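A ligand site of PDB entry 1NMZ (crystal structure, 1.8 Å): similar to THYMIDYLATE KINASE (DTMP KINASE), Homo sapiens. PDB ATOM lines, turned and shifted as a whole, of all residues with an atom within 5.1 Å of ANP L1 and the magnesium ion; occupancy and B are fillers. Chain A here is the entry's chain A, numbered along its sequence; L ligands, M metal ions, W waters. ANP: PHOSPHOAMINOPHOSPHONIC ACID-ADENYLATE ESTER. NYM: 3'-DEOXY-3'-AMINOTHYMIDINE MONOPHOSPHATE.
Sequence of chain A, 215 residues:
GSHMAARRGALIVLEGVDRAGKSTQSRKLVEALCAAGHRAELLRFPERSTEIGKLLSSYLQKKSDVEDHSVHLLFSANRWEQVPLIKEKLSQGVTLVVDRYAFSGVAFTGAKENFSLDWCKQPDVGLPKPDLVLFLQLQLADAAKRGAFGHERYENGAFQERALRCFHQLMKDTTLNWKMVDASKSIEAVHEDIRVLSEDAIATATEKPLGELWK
O2B of ANP L1 binds the magnesium ion. An oxygen (O2G) of ANP L1 is bound to the magnesium ion (2.1 Å). Water W8 is bound to the magnesium ion (2.1 Å). Water W9 binds the magnesium ion (2.1 Å). The magnesium ion is bound by water W13 (2.2 Å). The magnesium ion is bound by OG of Ser 23 (2.2 Å).
O2G of ANP L1 lies close to OP2 of NYM L2 (2.9 Å).
Water W9 bridges OD1 of Asp 99 (2.6 Å) and OP1 of NYM L2 (2.9 Å). Water W6 lies within hydrogen-bond range of O2' of ANP L1 (2.5 Å) and OG1 of Thr 24 (2.7 Å). Water W1 bridges a nitrogen (N7) of ANP L1 (2.7 Å) and the side-chain amide nitrogen of Gln 25 (2.8 Å). Water W11 bridges N1 of ANP L1 and O of Lys 185. Water W12 lies within hydrogen-bond range of O2A of ANP L1, NH2 of Arg 27 and OG1 of Thr 24.
One residue has an atom within 4 Å of the magnesium ion: Ser 23. The nearest printed residue that does not touch the magnesium ion is Asp 99 (4.2 Å).
The side-chain carboxylate (OD1) of Asp 18 sits close to an oxygen (O3G) of ANP L1, 3.4 Å away. The backbone NH of Ile 187 sits close to a nitrogen (N6) of ANP L1. Residues that only touch ANP L1: Ala 183 and Ser 186. Hydrophobic or aromatic side chains within 4 Å of ANP L1: Ile 187. Along chain A the residues within 4 Å of ANP L1 span positions 18 to 187.
O of Lys 185 is in hydrogen-bond range of N6 of ANP L1. An oxygen (O3G) of ANP L1 is in salt-bridge range of the side-chain amino group of Lys 22, 2.6 Å away. The backbone NH of Gly 21 sits at hydrogen-bond distance from an oxygen (O1B) of ANP L1, at 2.8 Å. An oxygen (O1A) of ANP L1 is in hydrogen-bond range of the backbone NH (N) of Thr 24. N of Ala 20 sits at hydrogen-bond distance from O1B of ANP L1. An oxygen (O3G) of ANP L1 sits at hydrogen-bond distance from the backbone NH (N) of Arg 19 (3.5 Å). O1B of ANP L1 is in hydrogen-bond range of N of Lys 22 (2.9 Å). OD1 of Asp 18 lies within salt-bridge range of N3' of NYM L2 (3.4 Å). NE of Arg 100 lies within salt-bridge range of OP1 of NYM L2, 2.8 Å away. O2B of ANP L1 lies close to N of Ser 23 (3.1 Å). The guanidinium group (NH2) of Arg 146 lies within hydrogen-bond range of a nitrogen (N1) of ANP L1, at 3.4 Å. The guanidinium group of Arg 100 lies within salt-bridge range of an oxygen (O3G) of ANP L1, at 2.8 Å. O1A of ANP L1 sits at hydrogen-bond distance from OG1 of Thr 24, 2.8 Å away.
The guanidinium group (NH2) of Arg 27 is in hydrogen-bond range of the side-chain hydroxyl (OG1) of Thr 24, 3.3 Å away. The backbone carbonyl oxygen (O) of Arg 146 lies within hydrogen-bond range of the guanidinium group (NH1) of Arg 19 (3.2 Å). O of Val 17 is in hydrogen-bond range of NZ of Lys 22, 2.9 Å away. The backbone carbonyl oxygen (O) of Ala 20 sits at hydrogen-bond distance from the guanidinium group (NH1) of Arg 146, 3.5 Å away. NH2 of Arg 146 is in hydrogen-bond range of O of Ala 183 (2.8 Å). The side-chain hydroxyl (OG) of Ser 23 lies close to the side-chain carboxylate (OD2) of Asp 99. The backbone carbonyl oxygen (O) of Ile 187 is in hydrogen-bond range of the side-chain amide nitrogen (NE2) of Gln 25.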
ATOM      1  N   VAL A  17      12.363 -14.621  20.755  1.00  0.00           N
ATOM      2  CA  VAL A  17      12.615 -14.368  19.336  1.00  0.00           C
ATOM      3  C   VAL A  17      14.117 -14.376  19.049  1.00  0.00           C
ATOM      4  O   VAL A  17      14.924 -14.306  19.980  1.00  0.00           O
ATOM      5  CB  VAL A  17      12.027 -12.990  18.925  1.00  0.00           C
ATOM      6  CG1 VAL A  17      10.520 -13.011  19.174  1.00  0.00           C
ATOM      7  CG2 VAL A  17      12.653 -11.816  19.674  1.00  0.00           C
ATOM      8  N   ASP A  18      14.494 -14.301  17.773  1.00  0.00           N
ATOM      9  CA  ASP A  18      15.934 -14.178  17.465  1.00  0.00           C
ATOM     10  C   ASP A  18      16.522 -12.924  18.103  1.00  0.00           C
ATOM     11  O   ASP A  18      16.017 -11.813  18.223  1.00  0.00           O
ATOM     12  CB  ASP A  18      16.140 -14.202  15.941  1.00  0.00           C
ATOM     13  CG  ASP A  18      15.607 -15.483  15.329  1.00  0.00           C
ATOM     14  OD1 ASP A  18      15.535 -16.533  15.995  1.00  0.00           O
ATOM     15  OD2 ASP A  18      15.233 -15.543  14.142  1.00  0.00           O
ATOM     16  N   ARG A  19      17.740 -13.095  18.611  1.00  0.00           N
ATOM     17  CA  ARG A  19      18.570 -12.095  19.257  1.00  0.00           C
ATOM     18  C   ARG A  19      18.150 -11.617  20.617  1.00  0.00           C
ATOM     19  O   ARG A  19      18.661 -10.630  21.147  1.00  0.00           O
ATOM     20  CB  ARG A  19      18.855 -10.850  18.396  1.00  0.00           C
ATOM     21  CG  ARG A  19      19.810 -11.189  17.248  1.00  0.00           C
ATOM     22  CD  ARG A  19      20.156  -9.942  16.453  1.00  0.00           C
ATOM     23  NE  ARG A  19      19.027  -9.502  15.643  1.00  0.00           N
ATOM     24  CZ  ARG A  19      18.938  -8.355  14.970  1.00  0.00           C
ATOM     25  NH1 ARG A  19      19.924  -7.465  15.001  1.00  0.00           N
ATOM     26  NH2 ARG A  19      17.852  -8.068  14.266  1.00  0.00           N
ATOM     27  N   ALA A  20      17.234 -12.344  21.252  1.00  0.00           N
ATOM     28  CA  ALA A  20      16.759 -12.017  22.572  1.00  0.00           C
ATOM     29  C   ALA A  20      17.810 -12.299  23.666  1.00  0.00           C
ATOM     30  O   ALA A  20      17.623 -11.817  24.763  1.00  0.00           O
ATOM     31  CB  ALA A  20      15.537 -12.882  22.895  1.00  0.00           C
ATOM     32  N   GLY A  21      18.865 -13.047  23.340  1.00  0.00           N
ATOM     33  CA  GLY A  21      19.851 -13.365  24.352  1.00  0.00           C
ATOM     34  C   GLY A  21      19.792 -14.801  24.851  1.00  0.00           C
ATOM     35  O   GLY A  21      20.436 -15.106  25.863  1.00  0.00           O
ATOM     36  N   LYS A  22      19.058 -15.675  24.189  1.00  0.00           N
ATOM     37  CA  LYS A  22      18.917 -17.056  24.644  1.00  0.00           C
ATOM     38  C   LYS A  22      20.219 -17.821  24.841  1.00  0.00           C
ATOM     39  O   LYS A  22      20.430 -18.535  25.830  1.00  0.00           O
ATOM     40  CB  LYS A  22      18.003 -17.837  23.675  1.00  0.00           C
ATOM     41  CG  LYS A  22      16.619 -17.125  23.591  1.00  0.00           C
ATOM     42  CD  LYS A  22      15.749 -17.901  22.560  1.00  0.00           C
ATOM     43  CE  LYS A  22      16.386 -17.973  21.176  1.00  0.00           C
ATOM     44  NZ  LYS A  22      16.492 -16.623  20.529  1.00  0.00           N
ATOM     45  N   SER A  23      21.101 -17.758  23.878  1.00  0.00           N
ATOM     46  CA  SER A  23      22.346 -18.526  23.912  1.00  0.00           C
ATOM     47  C   SER A  23      23.322 -17.955  24.964  1.00  0.00           C
ATOM     48  O   SER A  23      23.872 -18.765  25.709  1.00  0.00           O
ATOM     49  CB  SER A  23      22.975 -18.593  22.545  1.00  0.00           C
ATOM     50  OG  SER A  23      22.123 -19.273  21.630  1.00  0.00           O
ATOM     51  N   THR A  24      23.415 -16.639  24.999  1.00  0.00           N
ATOM     52  CA  THR A  24      24.299 -16.042  26.011  1.00  0.00           C
ATOM     53  C   THR A  24      23.785 -16.424  27.404  1.00  0.00           C
ATOM     54  O   THR A  24      24.550 -16.878  28.278  1.00  0.00           O
ATOM     55  CB  THR A  24      24.292 -14.525  25.829  1.00  0.00           C
ATOM     56  OG1 THR A  24      24.913 -14.145  24.585  1.00  0.00           O
ATOM     57  CG2 THR A  24      25.035 -13.884  27.018  1.00  0.00           C
ATOM     58  N   GLN A  25      22.457 -16.307  27.612  1.00  0.00           N
ATOM     59  CA  GLN A  25      21.891 -16.601  28.933  1.00  0.00           C
ATOM     60  C   GLN A  25      21.932 -18.080  29.250  1.00  0.00           C
ATOM     61  O   GLN A  25      22.129 -18.457  30.417  1.00  0.00           O
ATOM     62  CB  GLN A  25      20.471 -15.999  29.047  1.00  0.00           C
ATOM     63  CG  GLN A  25      20.435 -14.488  29.064  1.00  0.00           C
ATOM     64  CD  GLN A  25      21.303 -13.851  30.115  1.00  0.00           C
ATOM     65  OE1 GLN A  25      21.564 -14.406  31.184  1.00  0.00           O
ATOM     66  NE2 GLN A  25      21.773 -12.628  29.886  1.00  0.00           N
ATOM     67  N   ARG A  27      24.285 -20.292  28.309  1.00  0.00           N
ATOM     68  CA  ARG A  27      25.676 -20.563  28.675  1.00  0.00           C
ATOM     69  C   ARG A  27      26.009 -20.046  30.067  1.00  0.00           C
ATOM     70  O   ARG A  27      26.560 -20.783  30.916  1.00  0.00           O
ATOM     71  CB  ARG A  27      26.683 -19.877  27.679  1.00  0.00           C
ATOM     72  CG  ARG A  27      26.619 -20.522  26.264  1.00  0.00           C
ATOM     73  CD  ARG A  27      27.805 -19.883  25.510  1.00  0.00           C
ATOM     74  NE  ARG A  27      27.695 -18.443  25.330  1.00  0.00           N
ATOM     75  CZ  ARG A  27      27.109 -17.817  24.297  1.00  0.00           C
ATOM     76  NH1 ARG A  27      26.529 -18.482  23.305  1.00  0.00           N
ATOM     77  NH2 ARG A  27      27.155 -16.494  24.312  1.00  0.00           N
ATOM     78  N   ASP A  99      18.470 -24.369  25.177  1.00  0.00           N
ATOM     79  CA  ASP A  99      18.373 -23.164  24.345  1.00  0.00           C
ATOM     80  C   ASP A  99      17.461 -23.434  23.137  1.00  0.00           C
ATOM     81  O   ASP A  99      17.945 -24.063  22.175  1.00  0.00           O
ATOM     82  CB  ASP A  99      19.806 -22.836  23.943  1.00  0.00           C
ATOM     83  CG  ASP A  99      20.005 -21.608  23.085  1.00  0.00           C
ATOM     84  OD1 ASP A  99      19.081 -20.851  22.727  1.00  0.00           O
ATOM     85  OD2 ASP A  99      21.195 -21.495  22.642  1.00  0.00           O
ATOM     86  N   ARG A 100      16.220 -23.067  23.286  1.00  0.00           N
ATOM     87  CA  ARG A 100      15.109 -23.293  22.386  1.00  0.00           C
ATOM     88  C   ARG A 100      14.569 -24.724  22.539  1.00  0.00           C
ATOM     89  O   ARG A 100      15.354 -25.660  22.800  1.00  0.00           O
ATOM     90  CB  ARG A 100      15.333 -23.049  20.872  1.00  0.00           C
ATOM     91  CG  ARG A 100      15.715 -21.558  20.590  1.00  0.00           C
ATOM     92  CD  ARG A 100      15.622 -21.466  19.026  1.00  0.00           C
ATOM     93  NE  ARG A 100      16.030 -20.217  18.439  1.00  0.00           N
ATOM     94  CZ  ARG A 100      15.195 -19.199  18.217  1.00  0.00           C
ATOM     95  NH1 ARG A 100      13.915 -19.225  18.574  1.00  0.00           N
ATOM     96  NH2 ARG A 100      15.740 -18.114  17.654  1.00  0.00           N
ATOM     97  N   ARG A 146      20.530  -4.862  18.295  1.00  0.00           N
ATOM     98  CA  ARG A 146      21.600  -5.746  18.705  1.00  0.00           C
ATOM     99  C   ARG A 146      22.399  -6.130  17.465  1.00  0.00           C
ATOM    100  O   ARG A 146      22.370  -7.269  17.031  1.00  0.00           O
ATOM    101  CB  ARG A 146      21.176  -7.010  19.453  1.00  0.00           C
ATOM    102  CG  ARG A 146      21.019  -6.672  20.923  1.00  0.00           C
ATOM    103  CD  ARG A 146      20.117  -7.653  21.666  1.00  0.00           C
ATOM    104  NE  ARG A 146      19.689  -6.972  22.877  1.00  0.00           N
ATOM    105  CZ  ARG A 146      19.332  -7.607  23.984  1.00  0.00           C
ATOM    106  NH1 ARG A 146      19.379  -8.935  23.918  1.00  0.00           N
ATOM    107  NH2 ARG A 146      18.951  -6.912  25.035  1.00  0.00           N
ATOM    108  N   GLU A 155      15.298 -14.523   9.359  1.00  0.00           N
ATOM    109  CA  GLU A 155      15.859 -13.331   9.991  1.00  0.00           C
ATOM    110  C   GLU A 155      15.395 -12.048   9.310  1.00  0.00           C
ATOM    111  O   GLU A 155      16.171 -11.352   8.652  1.00  0.00           O
ATOM    112  CB  GLU A 155      17.383 -13.436  10.062  1.00  0.00           C
ATOM    113  CG  GLU A 155      17.792 -14.719  10.778  1.00  0.00           C
ATOM    114  CD  GLU A 155      19.193 -14.640  11.339  1.00  0.00           C
ATOM    115  OE1 GLU A 155      19.421 -15.187  12.438  1.00  0.00           O
ATOM    116  OE2 GLU A 155      20.040 -14.010  10.668  1.00  0.00           O
ATOM    117  N   ALA A 183      14.463  -9.066  28.959  1.00  0.00           N
ATOM    118  CA  ALA A 183      15.720  -9.288  28.258  1.00  0.00           C
ATOM    119  C   ALA A 183      16.360  -8.015  27.731  1.00  0.00           C
ATOM    120  O   ALA A 183      17.403  -8.100  27.103  1.00  0.00           O
ATOM    121  CB  ALA A 183      15.497 -10.322  27.147  1.00  0.00           C
ATOM    122  N   LYS A 185      17.498  -5.646  29.628  1.00  0.00           N
ATOM    123  CA  LYS A 185      18.508  -5.215  30.606  1.00  0.00           C
ATOM    124  C   LYS A 185      19.909  -5.688  30.236  1.00  0.00           C
ATOM    125  O   LYS A 185      20.074  -6.304  29.184  1.00  0.00           O
ATOM    126  CB  LYS A 185      18.032  -5.719  31.966  1.00  0.00           C
ATOM    127  CG  LYS A 185      16.646  -5.115  32.278  1.00  0.00           C
ATOM    128  CD  LYS A 185      16.279  -5.254  33.736  1.00  0.00           C
ATOM    129  CE  LYS A 185      16.327  -6.661  34.290  1.00  0.00           C
ATOM    130  NZ  LYS A 185      15.675  -6.835  35.627  1.00  0.00           N
ATOM    131  N   SER A 186      20.919  -5.400  31.028  1.00  0.00           N
ATOM    132  CA  SER A 186      22.287  -5.787  30.768  1.00  0.00           C
ATOM    133  C   SER A 186      22.416  -7.323  30.792  1.00  0.00           C
ATOM    134  O   SER A 186      21.597  -8.004  31.420  1.00  0.00           O
ATOM    135  CB  SER A 186      23.194  -5.189  31.832  1.00  0.00           C
ATOM    136  OG  SER A 186      23.173  -5.833  33.100  1.00  0.00           O
ATOM    137  N   ILE A 187      23.480  -7.835  30.184  1.00  0.00           N
ATOM    138  CA  ILE A 187      23.699  -9.295  30.246  1.00  0.00           C
ATOM    139  C   ILE A 187      23.723  -9.788  31.693  1.00  0.00           C
ATOM    140  O   ILE A 187      23.057 -10.776  32.023  1.00  0.00           O
ATOM    141  CB  ILE A 187      24.992  -9.678  29.519  1.00  0.00           C
ATOM    142  CG1 ILE A 187      24.701  -9.473  28.018  1.00  0.00           C
ATOM    143  CG2 ILE A 187      25.472 -11.078  29.851  1.00  0.00           C
ATOM    144  CD1 ILE A 187      25.963  -9.683  27.184  1.00  0.00           C
ATOM    145  N   VAL A 190      20.105  -9.475  33.423  1.00  0.00           N
ATOM    146  CA  VAL A 190      19.167 -10.510  32.929  1.00  0.00           C
ATOM    147  C   VAL A 190      19.592 -11.861  33.524  1.00  0.00           C
ATOM    148  O   VAL A 190      18.764 -12.663  33.925  1.00  0.00           O
ATOM    149  CB  VAL A 190      19.275 -10.555  31.384  1.00  0.00           C
ATOM    150  CG1 VAL A 190      18.473 -11.708  30.795  1.00  0.00           C
ATOM    151  CG2 VAL A 190      18.692  -9.246  30.849  1.00  0.00           C
HETATM  152  PG  ANP L   1      19.432 -16.430  18.088  1.00  0.00           P
HETATM  153  O1G ANP L   1      19.709 -15.805  16.735  1.00  0.00           O
HETATM  154  O2G ANP L   1      20.195 -17.658  18.180  1.00  0.00           O
HETATM  155  O3G ANP L   1      17.968 -16.573  18.349  1.00  0.00           O
HETATM  156  PB  ANP L   1      20.091 -15.417  20.778  1.00  0.00           P
HETATM  157  O1B ANP L   1      18.852 -15.061  21.389  1.00  0.00           O
HETATM  158  O2B ANP L   1      20.611 -16.756  21.022  1.00  0.00           O
HETATM  159  N3B ANP L   1      20.000 -15.221  19.080  1.00  0.00           N
HETATM  160  PA  ANP L   1      22.572 -14.238  21.641  1.00  0.00           P
HETATM  161  O1A ANP L   1      22.675 -14.676  23.071  1.00  0.00           O
HETATM  162  O2A ANP L   1      23.366 -14.995  20.661  1.00  0.00           O
HETATM  163  O3A ANP L   1      21.020 -14.202  21.247  1.00  0.00           O
HETATM  164  O5' ANP L   1      22.909 -12.694  21.593  1.00  0.00           O
HETATM  165  C5' ANP L   1      22.760 -11.944  20.312  1.00  0.00           C
HETATM  166  C4' ANP L   1      23.766 -10.797  20.346  1.00  0.00           C
HETATM  167  O4' ANP L   1      23.313  -9.819  21.271  1.00  0.00           O
HETATM  168  C3' ANP L   1      25.165 -11.188  20.819  1.00  0.00           C
HETATM  169  O3' ANP L   1      26.179 -10.304  20.217  1.00  0.00           O
HETATM  170  C2' ANP L   1      25.148 -10.927  22.293  1.00  0.00           C
HETATM  171  O2' ANP L   1      26.456 -10.580  22.845  1.00  0.00           O
HETATM  172  C1' ANP L   1      24.253  -9.680  22.356  1.00  0.00           C
HETATM  173  N9  ANP L   1      23.496  -9.637  23.636  1.00  0.00           N
HETATM  174  C8  ANP L   1      23.047 -10.682  24.400  1.00  0.00           C
HETATM  175  N7  ANP L   1      22.402 -10.298  25.479  1.00  0.00           N
HETATM  176  C5  ANP L   1      22.468  -8.927  25.435  1.00  0.00           C
HETATM  177  C6  ANP L   1      21.976  -7.936  26.320  1.00  0.00           C
HETATM  178  N6  ANP L   1      21.314  -8.243  27.467  1.00  0.00           N
HETATM  179  N1  ANP L   1      22.202  -6.670  25.968  1.00  0.00           N
HETATM  180  C2  ANP L   1      22.869  -6.389  24.840  1.00  0.00           C
HETATM  181  N3  ANP L   1      23.369  -7.219  23.943  1.00  0.00           N
HETATM  182  C4  ANP L   1      23.117  -8.501  24.311  1.00  0.00           C
HETATM  183  N1  NYM L   2      13.750 -22.986  14.699  1.00  0.00           N
HETATM  184  C6  NYM L   2      14.304 -23.532  15.810  1.00  0.00           C
HETATM  185  C2  NYM L   2      12.660 -23.551  13.985  1.00  0.00           C
HETATM  186  O2  NYM L   2      12.232 -22.999  12.963  1.00  0.00           O
HETATM  187  N3  NYM L   2      12.096 -24.646  14.543  1.00  0.00           N
HETATM  188  C4  NYM L   2      12.592 -25.262  15.703  1.00  0.00           C
HETATM  189  O4  NYM L   2      11.962 -26.370  16.097  1.00  0.00           O
HETATM  190  C5  NYM L   2      13.772 -24.629  16.370  1.00  0.00           C
HETATM  191  C7  NYM L   2      14.235 -25.374  17.635  1.00  0.00           C
HETATM  192  O4' NYM L   2      15.748 -22.228  13.927  1.00  0.00           O
HETATM  193  N3' NYM L   2      15.672 -18.909  13.584  1.00  0.00           N
HETATM  194  C1' NYM L   2      14.469 -21.816  14.084  1.00  0.00           C
HETATM  195  C2' NYM L   2      14.617 -20.587  15.000  1.00  0.00           C
HETATM  196  C3' NYM L   2      15.962 -19.982  14.631  1.00  0.00           C
HETATM  197  C4' NYM L   2      16.612 -21.115  13.827  1.00  0.00           C
HETATM  198  O5' NYM L   2      18.024 -21.095  15.763  1.00  0.00           O
HETATM  199  C5' NYM L   2      18.091 -21.321  14.321  1.00  0.00           C
HETATM  200  P1  NYM L   2      19.296 -20.680  16.667  1.00  0.00           P
HETATM  201  OP2 NYM L   2      20.197 -19.641  16.096  1.00  0.00           O
HETATM  202  OP1 NYM L   2      18.728 -20.670  18.016  1.00  0.00           O
HETATM  203  OP3 NYM L   2      20.223 -21.965  16.200  1.00  0.00           O
HETATM  204 MG    MG M   1      21.122 -18.328  19.919  1.00  0.00          MG
HETATM  205  O   HOH W   1      20.962 -11.301  27.523  1.00  0.00           O
HETATM  206  O   HOH W   2      26.488 -11.834  17.913  1.00  0.00           O
HETATM  207  O   HOH W   3      25.574 -14.467  18.874  1.00  0.00           O
HETATM  208  O   HOH W   4      27.143  -7.782  24.002  1.00  0.00           O
HETATM  209  O   HOH W   5      23.072 -17.248  16.441  1.00  0.00           O
HETATM  210  O   HOH W   6      27.102 -12.857  23.695  1.00  0.00           O
HETATM  211  O   HOH W   7      22.115 -13.887  17.310  1.00  0.00           O
HETATM  212  O   HOH W   8      22.922 -17.280  19.453  1.00  0.00           O
HETATM  213  O   HOH W   9      19.419 -19.475  20.510  1.00  0.00           O
HETATM  214  O   HOH W  10      24.626  -5.869  21.487  1.00  0.00           O
HETATM  215  O   HOH W  11      21.087  -4.412  27.100  1.00  0.00           O
HETATM  216  O   HOH W  12      25.833 -15.859  21.733  1.00  0.00           O
HETATM  217  O   HOH W  13      21.955 -20.014  18.821  1.00  0.00           O
